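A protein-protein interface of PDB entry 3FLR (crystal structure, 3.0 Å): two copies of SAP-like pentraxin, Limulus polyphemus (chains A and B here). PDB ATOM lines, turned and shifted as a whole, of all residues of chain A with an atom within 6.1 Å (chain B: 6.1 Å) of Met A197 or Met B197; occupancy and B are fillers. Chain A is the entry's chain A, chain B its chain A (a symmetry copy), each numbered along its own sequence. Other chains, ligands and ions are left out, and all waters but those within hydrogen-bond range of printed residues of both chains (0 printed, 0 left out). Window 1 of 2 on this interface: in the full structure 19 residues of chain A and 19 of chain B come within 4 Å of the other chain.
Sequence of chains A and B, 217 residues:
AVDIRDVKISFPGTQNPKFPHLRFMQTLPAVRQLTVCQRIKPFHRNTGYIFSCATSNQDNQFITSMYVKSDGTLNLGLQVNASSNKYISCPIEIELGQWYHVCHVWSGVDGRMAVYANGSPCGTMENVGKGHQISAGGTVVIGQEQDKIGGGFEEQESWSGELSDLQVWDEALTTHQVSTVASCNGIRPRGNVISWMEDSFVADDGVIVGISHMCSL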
ATOM      1  N   ILE A   4      30.525  18.045 -28.766  1.00  0.00           N
ATOM      2  CA  ILE A   4      30.134  18.582 -27.480  1.00  0.00           C
ATOM      3  C   ILE A   4      28.647  18.954 -27.419  1.00  0.00           C
ATOM      4  O   ILE A   4      28.032  18.930 -26.352  1.00  0.00           O
ATOM      5  CB  ILE A   4      30.998  19.823 -27.161  1.00  0.00           C
ATOM      6  CG1 ILE A   4      30.794  20.266 -25.725  1.00  0.00           C
ATOM      7  CG2 ILE A   4      30.626  20.967 -28.081  1.00  0.00           C
ATOM      8  CD1 ILE A   4      31.559  21.516 -25.401  1.00  0.00           C
ATOM      9  N   ARG A   5      28.062  19.284 -28.564  1.00  0.00           N
ATOM     10  CA  ARG A   5      26.657  19.679 -28.599  1.00  0.00           C
ATOM     11  C   ARG A   5      25.710  18.497 -28.474  1.00  0.00           C
ATOM     12  O   ARG A   5      24.511  18.678 -28.276  1.00  0.00           O
ATOM     13  CB  ARG A   5      26.369  20.454 -29.882  1.00  0.00           C
ATOM     14  CG  ARG A   5      27.283  21.652 -30.049  1.00  0.00           C
ATOM     15  CD  ARG A   5      27.065  22.349 -31.371  1.00  0.00           C
ATOM     16  NE  ARG A   5      25.641  22.593 -31.599  1.00  0.00           N
ATOM     17  CZ  ARG A   5      25.160  23.563 -32.375  1.00  0.00           C
ATOM     18  NH1 ARG A   5      26.002  24.383 -32.993  1.00  0.00           N
ATOM     19  NH2 ARG A   5      23.846  23.710 -32.533  1.00  0.00           N
ATOM     20  N   VAL A   7      25.924  16.273 -26.101  1.00  0.00           N
ATOM     21  CA  VAL A   7      25.870  15.843 -24.712  1.00  0.00           C
ATOM     22  C   VAL A   7      24.431  16.087 -24.283  1.00  0.00           C
ATOM     23  O   VAL A   7      23.816  17.070 -24.698  1.00  0.00           O
ATOM     24  CB  VAL A   7      26.800  16.677 -23.815  1.00  0.00           C
ATOM     25  CG1 VAL A   7      26.545  16.356 -22.373  1.00  0.00           C
ATOM     26  CG2 VAL A   7      28.229  16.373 -24.137  1.00  0.00           C
ATOM     27  N   LEU A 166      21.010  23.004 -25.998  1.00  0.00           N
ATOM     28  CA  LEU A 166      20.274  24.197 -25.587  1.00  0.00           C
ATOM     29  C   LEU A 166      21.007  25.444 -26.091  1.00  0.00           C
ATOM     30  O   LEU A 166      22.168  25.666 -25.744  1.00  0.00           O
ATOM     31  CB  LEU A 166      20.156  24.244 -24.057  1.00  0.00           C
ATOM     32  CG  LEU A 166      19.774  25.584 -23.410  1.00  0.00           C
ATOM     33  CD1 LEU A 166      18.374  25.978 -23.841  1.00  0.00           C
ATOM     34  CD2 LEU A 166      19.856  25.481 -21.897  1.00  0.00           C
ATOM     35  N   SER A 195      25.422  28.990 -24.875  1.00  0.00           N
ATOM     36  CA  SER A 195      25.808  27.958 -25.819  1.00  0.00           C
ATOM     37  C   SER A 195      25.977  26.679 -25.019  1.00  0.00           C
ATOM     38  O   SER A 195      26.788  26.611 -24.096  1.00  0.00           O
ATOM     39  CB  SER A 195      27.120  28.308 -26.518  1.00  0.00           C
ATOM     40  OG  SER A 195      27.479  27.269 -27.415  1.00  0.00           O
ATOM     41  N   TRP A 196      25.191  25.672 -25.377  1.00  0.00           N
ATOM     42  CA  TRP A 196      25.209  24.380 -24.699  1.00  0.00           C
ATOM     43  C   TRP A 196      26.630  23.899 -24.425  1.00  0.00           C
ATOM     44  O   TRP A 196      27.468  23.887 -25.319  1.00  0.00           O
ATOM     45  CB  TRP A 196      24.450  23.348 -25.542  1.00  0.00           C
ATOM     46  CG  TRP A 196      24.216  22.066 -24.847  1.00  0.00           C
ATOM     47  CD1 TRP A 196      24.565  20.825 -25.277  1.00  0.00           C
ATOM     48  CD2 TRP A 196      23.573  21.888 -23.587  1.00  0.00           C
ATOM     49  NE1 TRP A 196      24.181  19.875 -24.363  1.00  0.00           N
ATOM     50  CE2 TRP A 196      23.567  20.503 -23.314  1.00  0.00           C
ATOM     51  CE3 TRP A 196      23.000  22.766 -22.658  1.00  0.00           C
ATOM     52  CZ2 TRP A 196      23.009  19.973 -22.151  1.00  0.00           C
ATOM     53  CZ3 TRP A 196      22.446  22.243 -21.504  1.00  0.00           C
ATOM     54  CH2 TRP A 196      22.453  20.856 -21.257  1.00  0.00           C
ATOM     55  N   MET A 197      26.892  23.518 -23.178  1.00  0.00           N
ATOM     56  CA  MET A 197      28.204  23.029 -22.768  1.00  0.00           C
ATOM     57  C   MET A 197      29.298  24.090 -22.718  1.00  0.00           C
ATOM     58  O   MET A 197      30.289  23.919 -22.011  1.00  0.00           O
ATOM     59  CB  MET A 197      28.658  21.882 -23.671  1.00  0.00           C
ATOM     60  CG  MET A 197      27.783  20.651 -23.577  1.00  0.00           C
ATOM     61  SD  MET A 197      27.552  20.098 -21.873  1.00  0.00           S
ATOM     62  CE  MET A 197      28.815  18.881 -21.708  1.00  0.00           C
ATOM     63  N   GLU A 198      29.138  25.184 -23.457  1.00  0.00           N
ATOM     64  CA  GLU A 198      30.151  26.231 -23.430  1.00  0.00           C
ATOM     65  C   GLU A 198      29.989  27.137 -22.223  1.00  0.00           C
ATOM     66  O   GLU A 198      30.974  27.640 -21.693  1.00  0.00           O
ATOM     67  CB  GLU A 198      30.141  27.034 -24.727  1.00  0.00           C
ATOM     68  CG  GLU A 198      31.096  26.468 -25.774  1.00  0.00           C
ATOM     69  CD  GLU A 198      31.020  27.201 -27.101  1.00  0.00           C
ATOM     70  OE1 GLU A 198      31.196  28.442 -27.124  1.00  0.00           O
ATOM     71  OE2 GLU A 198      30.784  26.533 -28.129  1.00  0.00           O
ATOM     72  N   ASP A 199      28.755  27.352 -21.784  1.00  0.00           N
ATOM     73  CA  ASP A 199      28.521  28.163 -20.598  1.00  0.00           C
ATOM     74  C   ASP A 199      28.256  27.189 -19.464  1.00  0.00           C
ATOM     75  O   ASP A 199      27.328  26.380 -19.539  1.00  0.00           O
ATOM     76  CB  ASP A 199      27.331  29.074 -20.802  1.00  0.00           C
ATOM     77  CG  ASP A 199      27.601  30.129 -21.828  1.00  0.00           C
ATOM     78  OD1 ASP A 199      28.579  30.896 -21.662  1.00  0.00           O
ATOM     79  OD2 ASP A 199      26.836  30.188 -22.810  1.00  0.00           O
ATOM     80  N   SER A 200      29.080  27.263 -18.423  1.00  0.00           N
ATOM     81  CA  SER A 200      28.971  26.365 -17.283  1.00  0.00           C
ATOM     82  C   SER A 200      27.703  26.490 -16.466  1.00  0.00           C
ATOM     83  O   SER A 200      27.129  27.567 -16.339  1.00  0.00           O
ATOM     84  CB  SER A 200      30.175  26.548 -16.379  1.00  0.00           C
ATOM     85  OG  SER A 200      30.536  27.915 -16.321  1.00  0.00           O
ATOM     86  N   PHE A 201      27.282  25.366 -15.900  1.00  0.00           N
ATOM     87  CA  PHE A 201      26.074  25.304 -15.091  1.00  0.00           C
ATOM     88  C   PHE A 201      26.264  24.348 -13.916  1.00  0.00           C
ATOM     89  O   PHE A 201      27.220  23.573 -13.896  1.00  0.00           O
ATOM     90  CB  PHE A 201      24.907  24.848 -15.966  1.00  0.00           C
ATOM     91  CG  PHE A 201      25.122  23.514 -16.627  1.00  0.00           C
ATOM     92  CD1 PHE A 201      24.922  22.333 -15.926  1.00  0.00           C
ATOM     93  CD2 PHE A 201      25.495  23.440 -17.968  1.00  0.00           C
ATOM     94  CE1 PHE A 201      25.084  21.097 -16.554  1.00  0.00           C
ATOM     95  CE2 PHE A 201      25.662  22.210 -18.605  1.00  0.00           C
ATOM     96  CZ  PHE A 201      25.456  21.038 -17.901  1.00  0.00           C
ATOM     97  N   VAL A 209      24.113  12.394 -16.871  1.00  0.00           N
ATOM     98  CA  VAL A 209      24.801  13.011 -17.993  1.00  0.00           C
ATOM     99  C   VAL A 209      25.162  11.913 -18.978  1.00  0.00           C
ATOM    100  O   VAL A 209      25.737  10.890 -18.598  1.00  0.00           O
ATOM    101  CB  VAL A 209      26.080  13.734 -17.568  1.00  0.00           C
ATOM    102  CG1 VAL A 209      26.707  14.395 -18.773  1.00  0.00           C
ATOM    103  CG2 VAL A 209      25.770  14.760 -16.517  1.00  0.00           C
ATOM    104  N   GLY A 210      24.813  12.120 -20.241  1.00  0.00           N
ATOM    105  CA  GLY A 210      25.100  11.124 -21.254  1.00  0.00           C
ATOM    106  C   GLY A 210      25.227  11.741 -22.629  1.00  0.00           C
ATOM    107  O   GLY A 210      25.713  12.863 -22.770  1.00  0.00           O
ATOM    108  N   ILE A 211      24.782  11.005 -23.643  1.00  0.00           N
ATOM    109  CA  ILE A 211      24.851  11.462 -25.027  1.00  0.00           C
ATOM    110  C   ILE A 211      23.552  11.250 -25.817  1.00  0.00           C
ATOM    111  O   ILE A 211      22.904  10.215 -25.700  1.00  0.00           O
ATOM    112  CB  ILE A 211      26.016  10.767 -25.752  1.00  0.00           C
ATOM    113  CG1 ILE A 211      27.331  11.427 -25.328  1.00  0.00           C
ATOM    114  CG2 ILE A 211      25.796  10.797 -27.254  1.00  0.00           C
ATOM    115  CD1 ILE A 211      28.536  10.972 -26.111  1.00  0.00           C
ATOM    116  N   ILE B   4      34.481  16.629 -26.970  1.00  0.00           N
ATOM    117  CA  ILE B   4      33.766  16.049 -25.852  1.00  0.00           C
ATOM    118  C   ILE B   4      34.692  15.656 -24.694  1.00  0.00           C
ATOM    119  O   ILE B   4      34.281  15.641 -23.532  1.00  0.00           O
ATOM    120  CB  ILE B   4      32.978  14.812 -26.337  1.00  0.00           C
ATOM    121  CG1 ILE B   4      32.026  14.325 -25.261  1.00  0.00           C
ATOM    122  CG2 ILE B   4      33.934  13.690 -26.685  1.00  0.00           C
ATOM    123  CD1 ILE B   4      31.299  13.076 -25.668  1.00  0.00           C
ATOM    124  N   ARG B   5      35.946  15.352 -25.004  1.00  0.00           N
ATOM    125  CA  ARG B   5      36.892  14.940 -23.971  1.00  0.00           C
ATOM    126  C   ARG B   5      37.397  16.105 -23.136  1.00  0.00           C
ATOM    127  O   ARG B   5      38.029  15.903 -22.102  1.00  0.00           O
ATOM    128  CB  ARG B   5      38.064  14.198 -24.607  1.00  0.00           C
ATOM    129  CG  ARG B   5      37.612  13.018 -25.445  1.00  0.00           C
ATOM    130  CD  ARG B   5      38.767  12.356 -26.158  1.00  0.00           C
ATOM    131  NE  ARG B   5      39.870  12.100 -25.233  1.00  0.00           N
ATOM    132  CZ  ARG B   5      40.785  11.146 -25.400  1.00  0.00           C
ATOM    133  NH1 ARG B   5      40.718  10.356 -26.464  1.00  0.00           N
ATOM    134  NH2 ARG B   5      41.761  10.987 -24.508  1.00  0.00           N
ATOM    135  N   VAL B   7      35.426  18.262 -21.692  1.00  0.00           N
ATOM    136  CA  VAL B   7      34.400  18.651 -20.736  1.00  0.00           C
ATOM    137  C   VAL B   7      35.015  18.376 -19.371  1.00  0.00           C
ATOM    138  O   VAL B   7      35.743  17.397 -19.202  1.00  0.00           O
ATOM    139  CB  VAL B   7      33.126  17.805 -20.883  1.00  0.00           C
ATOM    140  CG1 VAL B   7      32.192  18.081 -19.743  1.00  0.00           C
ATOM    141  CG2 VAL B   7      32.437  18.137 -22.170  1.00  0.00           C
ATOM    142  N   LEU B 166      38.633  11.466 -18.087  1.00  0.00           N
ATOM    143  CA  LEU B 166      38.815  10.253 -17.295  1.00  0.00           C
ATOM    144  C   LEU B 166      38.738   9.030 -18.215  1.00  0.00           C
ATOM    145  O   LEU B 166      37.723   8.814 -18.878  1.00  0.00           O
ATOM    146  CB  LEU B 166      37.731  10.160 -16.212  1.00  0.00           C
ATOM    147  CG  LEU B 166      37.506   8.797 -15.540  1.00  0.00           C
ATOM    148  CD1 LEU B 166      38.748   8.397 -14.769  1.00  0.00           C
ATOM    149  CD2 LEU B 166      36.302   8.858 -14.616  1.00  0.00           C
ATOM    150  N   SER B 195      34.990   5.510 -20.880  1.00  0.00           N
ATOM    151  CA  SER B 195      35.442   6.573 -21.757  1.00  0.00           C
ATOM    152  C   SER B 195      34.708   7.831 -21.328  1.00  0.00           C
ATOM    153  O   SER B 195      33.478   7.883 -21.343  1.00  0.00           O
ATOM    154  CB  SER B 195      35.124   6.262 -23.218  1.00  0.00           C
ATOM    155  OG  SER B 195      35.559   7.330 -24.044  1.00  0.00           O
ATOM    156  N   TRP B 196      35.477   8.838 -20.935  1.00  0.00           N
ATOM    157  CA  TRP B 196      34.934  10.109 -20.471  1.00  0.00           C
ATOM    158  C   TRP B 196      33.795  10.601 -21.358  1.00  0.00           C
ATOM    159  O   TRP B 196      33.929  10.650 -22.576  1.00  0.00           O
ATOM    160  CB  TRP B 196      36.054  11.155 -20.413  1.00  0.00           C
ATOM    161  CG  TRP B 196      35.661  12.414 -19.747  1.00  0.00           C
ATOM    162  CD1 TRP B 196      35.744  13.670 -20.256  1.00  0.00           C
ATOM    163  CD2 TRP B 196      35.120  12.547 -18.435  1.00  0.00           C
ATOM    164  NE1 TRP B 196      35.287  14.589 -19.343  1.00  0.00           N
ATOM    165  CE2 TRP B 196      34.899  13.923 -18.212  1.00  0.00           C
ATOM    166  CE3 TRP B 196      34.799  11.635 -17.421  1.00  0.00           C
ATOM    167  CZ2 TRP B 196      34.371  14.412 -17.017  1.00  0.00           C
ATOM    168  CZ3 TRP B 196      34.277  12.117 -16.235  1.00  0.00           C
ATOM    169  CH2 TRP B 196      34.066  13.497 -16.040  1.00  0.00           C
ATOM    170  N   MET B 197      32.672  10.949 -20.736  1.00  0.00           N
ATOM    171  CA  MET B 197      31.502  11.444 -21.453  1.00  0.00           C
ATOM    172  C   MET B 197      30.766  10.396 -22.280  1.00  0.00           C
ATOM    173  O   MET B 197      29.583  10.560 -22.569  1.00  0.00           O
ATOM    174  CB  MET B 197      31.877  12.622 -22.351  1.00  0.00           C
ATOM    175  CG  MET B 197      32.358  13.838 -21.590  1.00  0.00           C
ATOM    176  SD  MET B 197      31.207  14.339 -20.290  1.00  0.00           S
ATOM    177  CE  MET B 197      30.244  15.568 -21.108  1.00  0.00           C
ATOM    178  N   GLU B 198      31.446   9.322 -22.671  1.00  0.00           N
ATOM    179  CA  GLU B 198      30.780   8.288 -23.454  1.00  0.00           C
ATOM    180  C   GLU B 198      29.981   7.346 -22.572  1.00  0.00           C
ATOM    181  O   GLU B 198      28.945   6.841 -22.989  1.00  0.00           O
ATOM    182  CB  GLU B 198      31.783   7.523 -24.312  1.00  0.00           C
ATOM    183  CG  GLU B 198      31.949   8.131 -25.701  1.00  0.00           C
ATOM    184  CD  GLU B 198      33.016   7.436 -26.526  1.00  0.00           C
ATOM    185  OE1 GLU B 198      32.936   6.198 -26.711  1.00  0.00           O
ATOM    186  OE2 GLU B 198      33.941   8.130 -26.996  1.00  0.00           O
ATOM    187  N   ASP B 199      30.454   7.102 -21.355  1.00  0.00           N
ATOM    188  CA  ASP B 199      29.716   6.255 -20.431  1.00  0.00           C
ATOM    189  C   ASP B 199      29.014   7.191 -19.464  1.00  0.00           C
ATOM    190  O   ASP B 199      29.664   7.991 -18.785  1.00  0.00           O
ATOM    191  CB  ASP B 199      30.656   5.334 -19.685  1.00  0.00           C
ATOM    192  CG  ASP B 199      31.274   4.312 -20.588  1.00  0.00           C
ATOM    193  OD1 ASP B 199      30.522   3.554 -21.244  1.00  0.00           O
ATOM    194  OD2 ASP B 199      32.518   4.271 -20.647  1.00  0.00           O
ATOM    195  N   SER B 200      27.688   7.099 -19.415  1.00  0.00           N
ATOM    196  CA  SER B 200      26.881   7.963 -18.566  1.00  0.00           C
ATOM    197  C   SER B 200      27.087   7.797 -17.076  1.00  0.00           C
ATOM    198  O   SER B 200      27.378   6.709 -16.588  1.00  0.00           O
ATOM    199  CB  SER B 200      25.414   7.769 -18.898  1.00  0.00           C
ATOM    200  OG  SER B 200      25.153   6.406 -19.174  1.00  0.00           O
ATOM    201  N   PHE B 201      26.916   8.898 -16.356  1.00  0.00           N
ATOM    202  CA  PHE B 201      27.086   8.922 -14.911  1.00  0.00           C
ATOM    203  C   PHE B 201      26.057   9.845 -14.264  1.00  0.00           C
ATOM    204  O   PHE B 201      25.410  10.632 -14.954  1.00  0.00           O
ATOM    205  CB  PHE B 201      28.504   9.386 -14.579  1.00  0.00           C
ATOM    206  CG  PHE B 201      28.849  10.742 -15.134  1.00  0.00           C
ATOM    207  CD1 PHE B 201      28.431  11.899 -14.493  1.00  0.00           C
ATOM    208  CD2 PHE B 201      29.623  10.859 -16.287  1.00  0.00           C
ATOM    209  CE1 PHE B 201      28.785  13.155 -14.988  1.00  0.00           C
ATOM    210  CE2 PHE B 201      29.983  12.110 -16.793  1.00  0.00           C
ATOM    211  CZ  PHE B 201      29.566  13.257 -16.144  1.00  0.00           C
ATOM    212  N   VAL B 209      29.543  21.849 -14.207  1.00  0.00           N
ATOM    213  CA  VAL B 209      29.956  21.275 -15.477  1.00  0.00           C
ATOM    214  C   VAL B 209      30.454  22.406 -16.359  1.00  0.00           C
ATOM    215  O   VAL B 209      29.778  23.424 -16.519  1.00  0.00           O
ATOM    216  CB  VAL B 209      28.810  20.557 -16.192  1.00  0.00           C
ATOM    217  CG1 VAL B 209      29.326  19.939 -17.470  1.00  0.00           C
ATOM    218  CG2 VAL B 209      28.227  19.497 -15.304  1.00  0.00           C
ATOM    219  N   GLY B 210      31.643  22.230 -16.921  1.00  0.00           N
ATOM    220  CA  GLY B 210      32.213  23.259 -17.768  1.00  0.00           C
ATOM    221  C   GLY B 210      33.182  22.683 -18.776  1.00  0.00           C
ATOM    222  O   GLY B 210      32.989  21.571 -19.269  1.00  0.00           O
ATOM    223  N   ILE B 211      34.232  23.442 -19.075  1.00  0.00           N
ATOM    224  CA  ILE B 211      35.245  23.026 -20.041  1.00  0.00           C
ATOM    225  C   ILE B 211      36.686  23.243 -19.562  1.00  0.00           C
ATOM    226  O   ILE B 211      37.005  24.266 -18.963  1.00  0.00           O
ATOM    227  CB  ILE B 211      35.028  23.757 -21.377  1.00  0.00           C
ATOM    228  CG1 ILE B 211      33.860  23.102 -22.119  1.00  0.00           C
ATOM    229  CG2 ILE B 211      36.313  23.767 -22.187  1.00  0.00           C
ATOM    230  CD1 ILE B 211      33.665  23.595 -23.530  1.00  0.00           C
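Printed residues of chain A that touch a printed residue of chain B: Ile A4, Val A7, Met A197, Ser A200, Phe A201, Val A209 and Ile A211. Along chain A the printed residues that touch a printed residue of chain B span positions 4 to 211. Among the printed residues, 11 pairs touch across the chains. Among the printed residues, no Asp or Glu carboxylate lies within 4 Å of a Lys or Arg side-chain nitrogen of the other chain.
Among the printed residues, merely in contact across the chains: Ile A4 with Ile B211 (3.5 Å), Val A7 with Met B197 (3.7 Å), Met A197 with Val B7 (3.7 Å), Met A197 with Met B197 (3.7 Å), Met A197 with Ile B211 (3.7 Å), Ser A200 with Val B209 (3.1 Å), Val A209 with Ser B200 (3.1 Å), Ile A211 with Ile B4 (3.5 Å) and Ile A211 with Met B197 (3.7 Å).
The backbone carbonyl oxygen (O) of Val B7 sits at hydrogen-bond distance from the indole nitrogen (NE1) of Trp B196, 2.8 Å away. O of Val A7 sits at hydrogen-bond distance from NE1 of Trp A196, 2.8 Å away.
The backbone carbonyl oxygen (O) of Phe A201 sits at hydrogen-bond distance from the backbone NH (N) of Val B209. O of Phe B201 sits at hydrogen-bond distance from N of Val A209 (2.9 Å).
Ile A4 touches Ile B211, and with the chains exchanged Ile A211 touches Ile B4. Met B197 touches its own counterpart, Met A197. Met A197 touches Ile B211, and with the chains exchanged Ile A211 touches Met B197. Phe A201 touches Val B209, and with the chains exchanged Val A209 touches Phe B201. 14 positions are printed for both chains. Of the 11 pairs that touch across the chains among the printed residues, 11 have their exchanged pair printed and touching as well.
Of the printed residues of chain B, Ile A4 touches Ile B211 (3.5 Å). Met A197 touches just these residues of chain B: Val B7, Met B197 and Ile B211. Of the printed residues of chain B, Ser A200 touches Val B209. Met B197 touches just these residues of chain A: Val A7, Met A197 and Ile A211. Printed residues of chain A within 4 Å of Val B209: Ser A200 and Phe A201. The nearest residue of chain B that does not touch Met A197 is Val B209 (4.4 Å). The nearest printed residue of chain A that does not touch Ser B200 is Gly A210 (4.1 Å).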
